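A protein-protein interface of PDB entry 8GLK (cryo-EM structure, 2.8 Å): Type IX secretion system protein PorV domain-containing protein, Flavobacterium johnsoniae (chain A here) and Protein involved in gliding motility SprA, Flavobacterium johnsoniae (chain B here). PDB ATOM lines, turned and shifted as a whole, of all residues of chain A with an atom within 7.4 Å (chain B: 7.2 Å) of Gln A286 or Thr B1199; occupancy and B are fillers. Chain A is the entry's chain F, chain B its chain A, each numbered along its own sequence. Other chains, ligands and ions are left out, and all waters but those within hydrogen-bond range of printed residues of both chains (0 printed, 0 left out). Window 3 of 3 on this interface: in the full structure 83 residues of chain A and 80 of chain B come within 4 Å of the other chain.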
ATOM      1  N   SER A 283      25.122  12.243 -17.914  1.00  0.00           N
ATOM      2  CA  SER A 283      25.492  13.470 -17.219  1.00  0.00           C
ATOM      3  C   SER A 283      24.680  14.654 -17.730  1.00  0.00           C
ATOM      4  O   SER A 283      23.474  14.543 -17.952  1.00  0.00           O
ATOM      5  CB  SER A 283      26.989  13.747 -17.382  1.00  0.00           C
ATOM      6  OG  SER A 283      27.304  14.077 -18.722  1.00  0.00           O
ATOM      7  N   GLN A 284      25.349  15.792 -17.914  1.00  0.00           N
ATOM      8  CA  GLN A 284      24.688  17.004 -18.388  1.00  0.00           C
ATOM      9  C   GLN A 284      24.626  17.045 -19.913  1.00  0.00           C
ATOM     10  O   GLN A 284      23.544  17.168 -20.495  1.00  0.00           O
ATOM     11  CB  GLN A 284      25.409  18.241 -17.841  1.00  0.00           C
ATOM     12  CG  GLN A 284      25.457  18.305 -16.323  1.00  0.00           C
ATOM     13  CD  GLN A 284      24.084  18.494 -15.705  1.00  0.00           C
ATOM     14  OE1 GLN A 284      23.226  19.173 -16.268  1.00  0.00           O
ATOM     15  NE2 GLN A 284      23.871  17.891 -14.541  1.00  0.00           N
ATOM     16  N   SER A 285      25.783  16.943 -20.571  1.00  0.00           N
ATOM     17  CA  SER A 285      25.818  16.917 -22.027  1.00  0.00           C
ATOM     18  C   SER A 285      25.384  15.575 -22.600  1.00  0.00           C
ATOM     19  O   SER A 285      25.034  15.506 -23.783  1.00  0.00           O
ATOM     20  CB  SER A 285      27.225  17.258 -22.525  1.00  0.00           C
ATOM     21  OG  SER A 285      28.187  16.374 -21.977  1.00  0.00           O
ATOM     22  N   GLN A 286      25.398  14.512 -21.790  1.00  0.00           N
ATOM     23  CA  GLN A 286      25.019  13.196 -22.290  1.00  0.00           C
ATOM     24  C   GLN A 286      23.546  13.150 -22.674  1.00  0.00           C
ATOM     25  O   GLN A 286      23.173  12.471 -23.637  1.00  0.00           O
ATOM     26  CB  GLN A 286      25.338  12.124 -21.247  1.00  0.00           C
ATOM     27  CG  GLN A 286      26.823  11.862 -21.063  1.00  0.00           C
ATOM     28  CD  GLN A 286      27.100  10.778 -20.040  1.00  0.00           C
ATOM     29  OE1 GLN A 286      26.201  10.342 -19.322  1.00  0.00           O
ATOM     30  NE2 GLN A 286      28.350  10.337 -19.969  1.00  0.00           N
ATOM     31  N   ALA A 287      22.691  13.858 -21.931  1.00  0.00           N
ATOM     32  CA  ALA A 287      21.276  13.904 -22.284  1.00  0.00           C
ATOM     33  C   ALA A 287      21.067  14.552 -23.647  1.00  0.00           C
ATOM     34  O   ALA A 287      20.307  14.041 -24.478  1.00  0.00           O
ATOM     35  CB  ALA A 287      20.489  14.650 -21.207  1.00  0.00           C
ATOM     36  N   ASP A 288      21.745  15.676 -23.899  1.00  0.00           N
ATOM     37  CA  ASP A 288      21.638  16.332 -25.198  1.00  0.00           C
ATOM     38  C   ASP A 288      22.213  15.458 -26.305  1.00  0.00           C
ATOM     39  O   ASP A 288      21.661  15.398 -27.410  1.00  0.00           O
ATOM     40  CB  ASP A 288      22.345  17.686 -25.160  1.00  0.00           C
ATOM     41  CG  ASP A 288      21.975  18.502 -23.939  1.00  0.00           C
ATOM     42  OD1 ASP A 288      20.862  18.309 -23.408  1.00  0.00           O
ATOM     43  OD2 ASP A 288      22.799  19.337 -23.509  1.00  0.00           O
ATOM     44  N   GLU A 289      23.328  14.777 -26.029  1.00  0.00           N
ATOM     45  CA  GLU A 289      23.912  13.879 -27.020  1.00  0.00           C
ATOM     46  C   GLU A 289      22.950  12.752 -27.376  1.00  0.00           C
ATOM     47  O   GLU A 289      22.770  12.429 -28.555  1.00  0.00           O
ATOM     48  CB  GLU A 289      25.232  13.311 -26.503  1.00  0.00           C
ATOM     49  CG  GLU A 289      26.385  14.300 -26.508  1.00  0.00           C
ATOM     50  CD  GLU A 289      27.630  13.743 -25.845  1.00  0.00           C
ATOM     51  OE1 GLU A 289      27.555  12.634 -25.277  1.00  0.00           O
ATOM     52  OE2 GLU A 289      28.681  14.415 -25.892  1.00  0.00           O
ATOM     53  N   ALA A 290      22.322  12.146 -26.366  1.00  0.00           N
ATOM     54  CA  ALA A 290      21.361  11.076 -26.619  1.00  0.00           C
ATOM     55  C   ALA A 290      20.148  11.593 -27.380  1.00  0.00           C
ATOM     56  O   ALA A 290      19.649  10.920 -28.291  1.00  0.00           O
ATOM     57  CB  ALA A 290      20.936  10.429 -25.302  1.00  0.00           C
ATOM     58  N   ASN A 291      19.659  12.784 -27.025  1.00  0.00           N
ATOM     59  CA  ASN A 291      18.519  13.354 -27.732  1.00  0.00           C
ATOM     60  C   ASN A 291      18.847  13.604 -29.199  1.00  0.00           C
ATOM     61  O   ASN A 291      18.046  13.285 -30.086  1.00  0.00           O
ATOM     62  CB  ASN A 291      18.074  14.648 -27.053  1.00  0.00           C
ATOM     63  CG  ASN A 291      17.287  14.399 -25.782  1.00  0.00           C
ATOM     64  OD1 ASN A 291      17.429  15.125 -24.799  1.00  0.00           O
ATOM     65  ND2 ASN A 291      16.450  13.369 -25.798  1.00  0.00           N
ATOM     66  N   TYR A 292      20.027  14.163 -29.477  1.00  0.00           N
ATOM     67  CA  TYR A 292      20.402  14.430 -30.861  1.00  0.00           C
ATOM     68  C   TYR A 292      20.638  13.137 -31.632  1.00  0.00           C
ATOM     69  O   TYR A 292      20.301  13.047 -32.819  1.00  0.00           O
ATOM     70  CB  TYR A 292      21.641  15.322 -30.916  1.00  0.00           C
ATOM     71  CG  TYR A 292      21.903  15.893 -32.289  1.00  0.00           C
ATOM     72  CD1 TYR A 292      21.112  16.915 -32.799  1.00  0.00           C
ATOM     73  CD2 TYR A 292      22.934  15.406 -33.081  1.00  0.00           C
ATOM     74  CE1 TYR A 292      21.344  17.439 -34.057  1.00  0.00           C
ATOM     75  CE2 TYR A 292      23.173  15.923 -34.340  1.00  0.00           C
ATOM     76  CZ  TYR A 292      22.375  16.940 -34.822  1.00  0.00           C
ATOM     77  OH  TYR A 292      22.611  17.458 -36.075  1.00  0.00           O
ATOM     78  N   LYS A 293      21.220  12.127 -30.981  1.00  0.00           N
ATOM     79  CA  LYS A 293      21.407  10.835 -31.634  1.00  0.00           C
ATOM     80  C   LYS A 293      20.068  10.197 -31.978  1.00  0.00           C
ATOM     81  O   LYS A 293      19.907   9.615 -33.057  1.00  0.00           O
ATOM     82  CB  LYS A 293      22.232   9.911 -30.739  1.00  0.00           C
ATOM     83  CG  LYS A 293      22.474   8.528 -31.319  1.00  0.00           C
ATOM     84  CD  LYS A 293      23.313   7.681 -30.377  1.00  0.00           C
ATOM     85  CE  LYS A 293      23.550   6.289 -30.940  1.00  0.00           C
ATOM     86  NZ  LYS A 293      24.448   5.486 -30.065  1.00  0.00           N
ATOM     87  N   GLU B1197      33.533  15.199 -23.048  1.00  0.00           N
ATOM     88  CA  GLU B1197      33.424  13.749 -23.116  1.00  0.00           C
ATOM     89  C   GLU B1197      32.222  13.390 -23.979  1.00  0.00           C
ATOM     90  O   GLU B1197      31.096  13.803 -23.683  1.00  0.00           O
ATOM     91  CB  GLU B1197      33.292  13.146 -21.718  1.00  0.00           C
ATOM     92  CG  GLU B1197      34.539  13.303 -20.863  1.00  0.00           C
ATOM     93  CD  GLU B1197      34.374  12.715 -19.476  1.00  0.00           C
ATOM     94  OE1 GLU B1197      33.249  12.295 -19.137  1.00  0.00           O
ATOM     95  OE2 GLU B1197      35.371  12.675 -18.724  1.00  0.00           O
ATOM     96  N   VAL B1198      32.464  12.629 -25.044  1.00  0.00           N
ATOM     97  CA  VAL B1198      31.426  12.194 -25.967  1.00  0.00           C
ATOM     98  C   VAL B1198      31.176  10.715 -25.713  1.00  0.00           C
ATOM     99  O   VAL B1198      32.112   9.907 -25.739  1.00  0.00           O
ATOM    100  CB  VAL B1198      31.830  12.446 -27.429  1.00  0.00           C
ATOM    101  CG1 VAL B1198      30.722  12.007 -28.367  1.00  0.00           C
ATOM    102  CG2 VAL B1198      32.176  13.910 -27.642  1.00  0.00           C
ATOM    103  N   THR B1199      29.914  10.362 -25.474  1.00  0.00           N
ATOM    104  CA  THR B1199      29.574   9.026 -24.994  1.00  0.00           C
ATOM    105  C   THR B1199      29.195   8.082 -26.133  1.00  0.00           C
ATOM    106  O   THR B1199      29.778   7.002 -26.273  1.00  0.00           O
ATOM    107  CB  THR B1199      28.435   9.116 -23.973  1.00  0.00           C
ATOM    108  OG1 THR B1199      28.848   9.928 -22.867  1.00  0.00           O
ATOM    109  CG2 THR B1199      28.063   7.733 -23.467  1.00  0.00           C
ATOM    110  N   ASN B1200      28.225   8.473 -26.950  1.00  0.00           N
ATOM    111  CA  ASN B1200      27.652   7.608 -27.980  1.00  0.00           C
ATOM    112  C   ASN B1200      28.080   8.109 -29.359  1.00  0.00           C
ATOM    113  O   ASN B1200      27.405   8.932 -29.979  1.00  0.00           O
ATOM    114  CB  ASN B1200      26.129   7.547 -27.833  1.00  0.00           C
ATOM    115  CG  ASN B1200      25.498   8.922 -27.679  1.00  0.00           C
ATOM    116  OD1 ASN B1200      26.179   9.945 -27.752  1.00  0.00           O
ATOM    117  ND2 ASN B1200      24.190   8.948 -27.454  1.00  0.00           N
ATOM    118  N   VAL B1201      29.210   7.598 -29.838  1.00  0.00           N
ATOM    119  CA  VAL B1201      29.719   7.915 -31.167  1.00  0.00           C
ATOM    120  C   VAL B1201      29.271   6.818 -32.122  1.00  0.00           C
ATOM    121  O   VAL B1201      29.560   5.637 -31.903  1.00  0.00           O
ATOM    122  CB  VAL B1201      31.249   8.051 -31.168  1.00  0.00           C
ATOM    123  CG1 VAL B1201      31.744   8.445 -32.552  1.00  0.00           C
ATOM    124  CG2 VAL B1201      31.695   9.063 -30.134  1.00  0.00           C
ATOM    125  N   ASP B1202      28.565   7.204 -33.182  1.00  0.00           N
ATOM    126  CA  ASP B1202      28.152   6.247 -34.200  1.00  0.00           C
ATOM    127  C   ASP B1202      29.338   5.898 -35.089  1.00  0.00           C
ATOM    128  O   ASP B1202      30.025   6.787 -35.601  1.00  0.00           O
ATOM    129  CB  ASP B1202      27.006   6.813 -35.034  1.00  0.00           C
ATOM    130  CG  ASP B1202      25.678   6.763 -34.308  1.00  0.00           C
ATOM    131  OD1 ASP B1202      25.421   5.762 -33.608  1.00  0.00           O
ATOM    132  OD2 ASP B1202      24.892   7.724 -34.438  1.00  0.00           O
ATOM    133  N   THR B1208      29.619   1.401 -31.223  1.00  0.00           N
ATOM    134  CA  THR B1208      29.731   2.692 -30.563  1.00  0.00           C
ATOM    135  C   THR B1208      31.024   2.744 -29.764  1.00  0.00           C
ATOM    136  O   THR B1208      31.554   1.712 -29.343  1.00  0.00           O
ATOM    137  CB  THR B1208      28.537   2.968 -29.633  1.00  0.00           C
ATOM    138  OG1 THR B1208      28.340   1.850 -28.758  1.00  0.00           O
ATOM    139  CG2 THR B1208      27.270   3.206 -30.442  1.00  0.00           C
ATOM    140  N   THR B1209      31.530   3.958 -29.562  1.00  0.00           N
ATOM    141  CA  THR B1209      32.777   4.161 -28.840  1.00  0.00           C
ATOM    142  C   THR B1209      32.693   5.444 -28.027  1.00  0.00           C
ATOM    143  O   THR B1209      31.864   6.318 -28.286  1.00  0.00           O
ATOM    144  CB  THR B1209      33.984   4.217 -29.789  1.00  0.00           C
ATOM    145  OG1 THR B1209      35.197   4.152 -29.030  1.00  0.00           O
ATOM    146  CG2 THR B1209      33.970   5.504 -30.601  1.00  0.00           C
ATOM    147  N   ASN B1210      33.562   5.536 -27.027  1.00  0.00           N
ATOM    148  CA  ASN B1210      33.689   6.722 -26.195  1.00  0.00           C
ATOM    149  C   ASN B1210      34.859   7.570 -26.680  1.00  0.00           C
ATOM    150  O   ASN B1210      35.867   7.050 -27.163  1.00  0.00           O
ATOM    151  CB  ASN B1210      33.896   6.341 -24.729  1.00  0.00           C
ATOM    152  CG  ASN B1210      32.603   5.951 -24.040  1.00  0.00           C
ATOM    153  OD1 ASN B1210      31.657   6.734 -23.983  1.00  0.00           O
ATOM    154  ND2 ASN B1210      32.558   4.733 -23.515  1.00  0.00           N
ATOM    155  N   ALA B1211      34.715   8.886 -26.548  1.00  0.00           N
ATOM    156  CA  ALA B1211      35.752   9.815 -26.972  1.00  0.00           C
ATOM    157  C   ALA B1211      35.893  10.921 -25.938  1.00  0.00           C
ATOM    158  O   ALA B1211      34.968  11.211 -25.178  1.00  0.00           O
ATOM    159  CB  ALA B1211      35.450  10.410 -28.352  1.00  0.00           C
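The side-chain hydroxyl of Thr B1199 is in hydrogen-bond range of the side-chain amide nitrogen of Gln A286 (3.0 Å). OE1 of Glu A289 sits at hydrogen-bond distance from N of Thr B1199. OD1 of Asp B1202 is in salt-bridge range of NZ of Lys A293 (3.7 Å). The side-chain carboxylate (OE2) of Glu A289 sits close to the backbone carbonyl oxygen (O) of Glu B1197 (3.3 Å).
The backbone NH (N) of Val B1198 sits at hydrogen-bond distance from the backbone carbonyl oxygen (O) of Ala B1211 (2.9 Å). OD1 of Asn B1210 sits close to O of Thr B1199, 3.0 Å away. The backbone NH of Ser A283 sits at hydrogen-bond distance from the side-chain amide oxygen of Gln A286 (2.6 Å).
Ala A287 touches none of the printed residues of chain B. Of the printed residues of chain B, Lys A293 touches Asn B1200, Asp B1202 and Thr B1208. Of the printed residues of chain A, Val B1198 touches Glu A289 (3.5 Å). Thr B1199 touches two residues of chain A. Printed residues of chain A within 4 Å of Asn B1200: Glu A289 (3.7 Å), Ala A290 (3.6 Å) and Lys A293 (3.3 Å). Of the printed residues of chain A, Asp B1202 touches Lys A293 (3.3 Å). The nearest residue of chain B that does not touch Gln A286 is Asn B1200 (5.3 Å). The nearest residue of chain A that does not touch Thr B1199 is Ser A283 (6.1 Å).
Of the 10 printed residues of chain B, 6 touch a printed residue of chain A. Printed residues of chain B that touch a printed residue of chain A: Glu B1197, Val B1198, Thr B1199, Asn B1200, Asp B1202 and Thr B1208. Hydrophobic or aromatic side chains of chain B that line the printed part of chain A: Val B1198. Among the printed residues, 9 pairs touch across the chains. Among the printed residues, Asp or Glu carboxylates within 4 Å of a Lys or Arg side-chain nitrogen of the other chain: Lys A293 with Asp B1202 (3.7 Å).
Among the printed residues, merely in contact across the chains: Glu A289 with Val B1198, Glu A289 with Asn B1200, Ala A290 with Asn B1200, Lys A293 with Asn B1200 and Lys A293 with Thr B1208.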
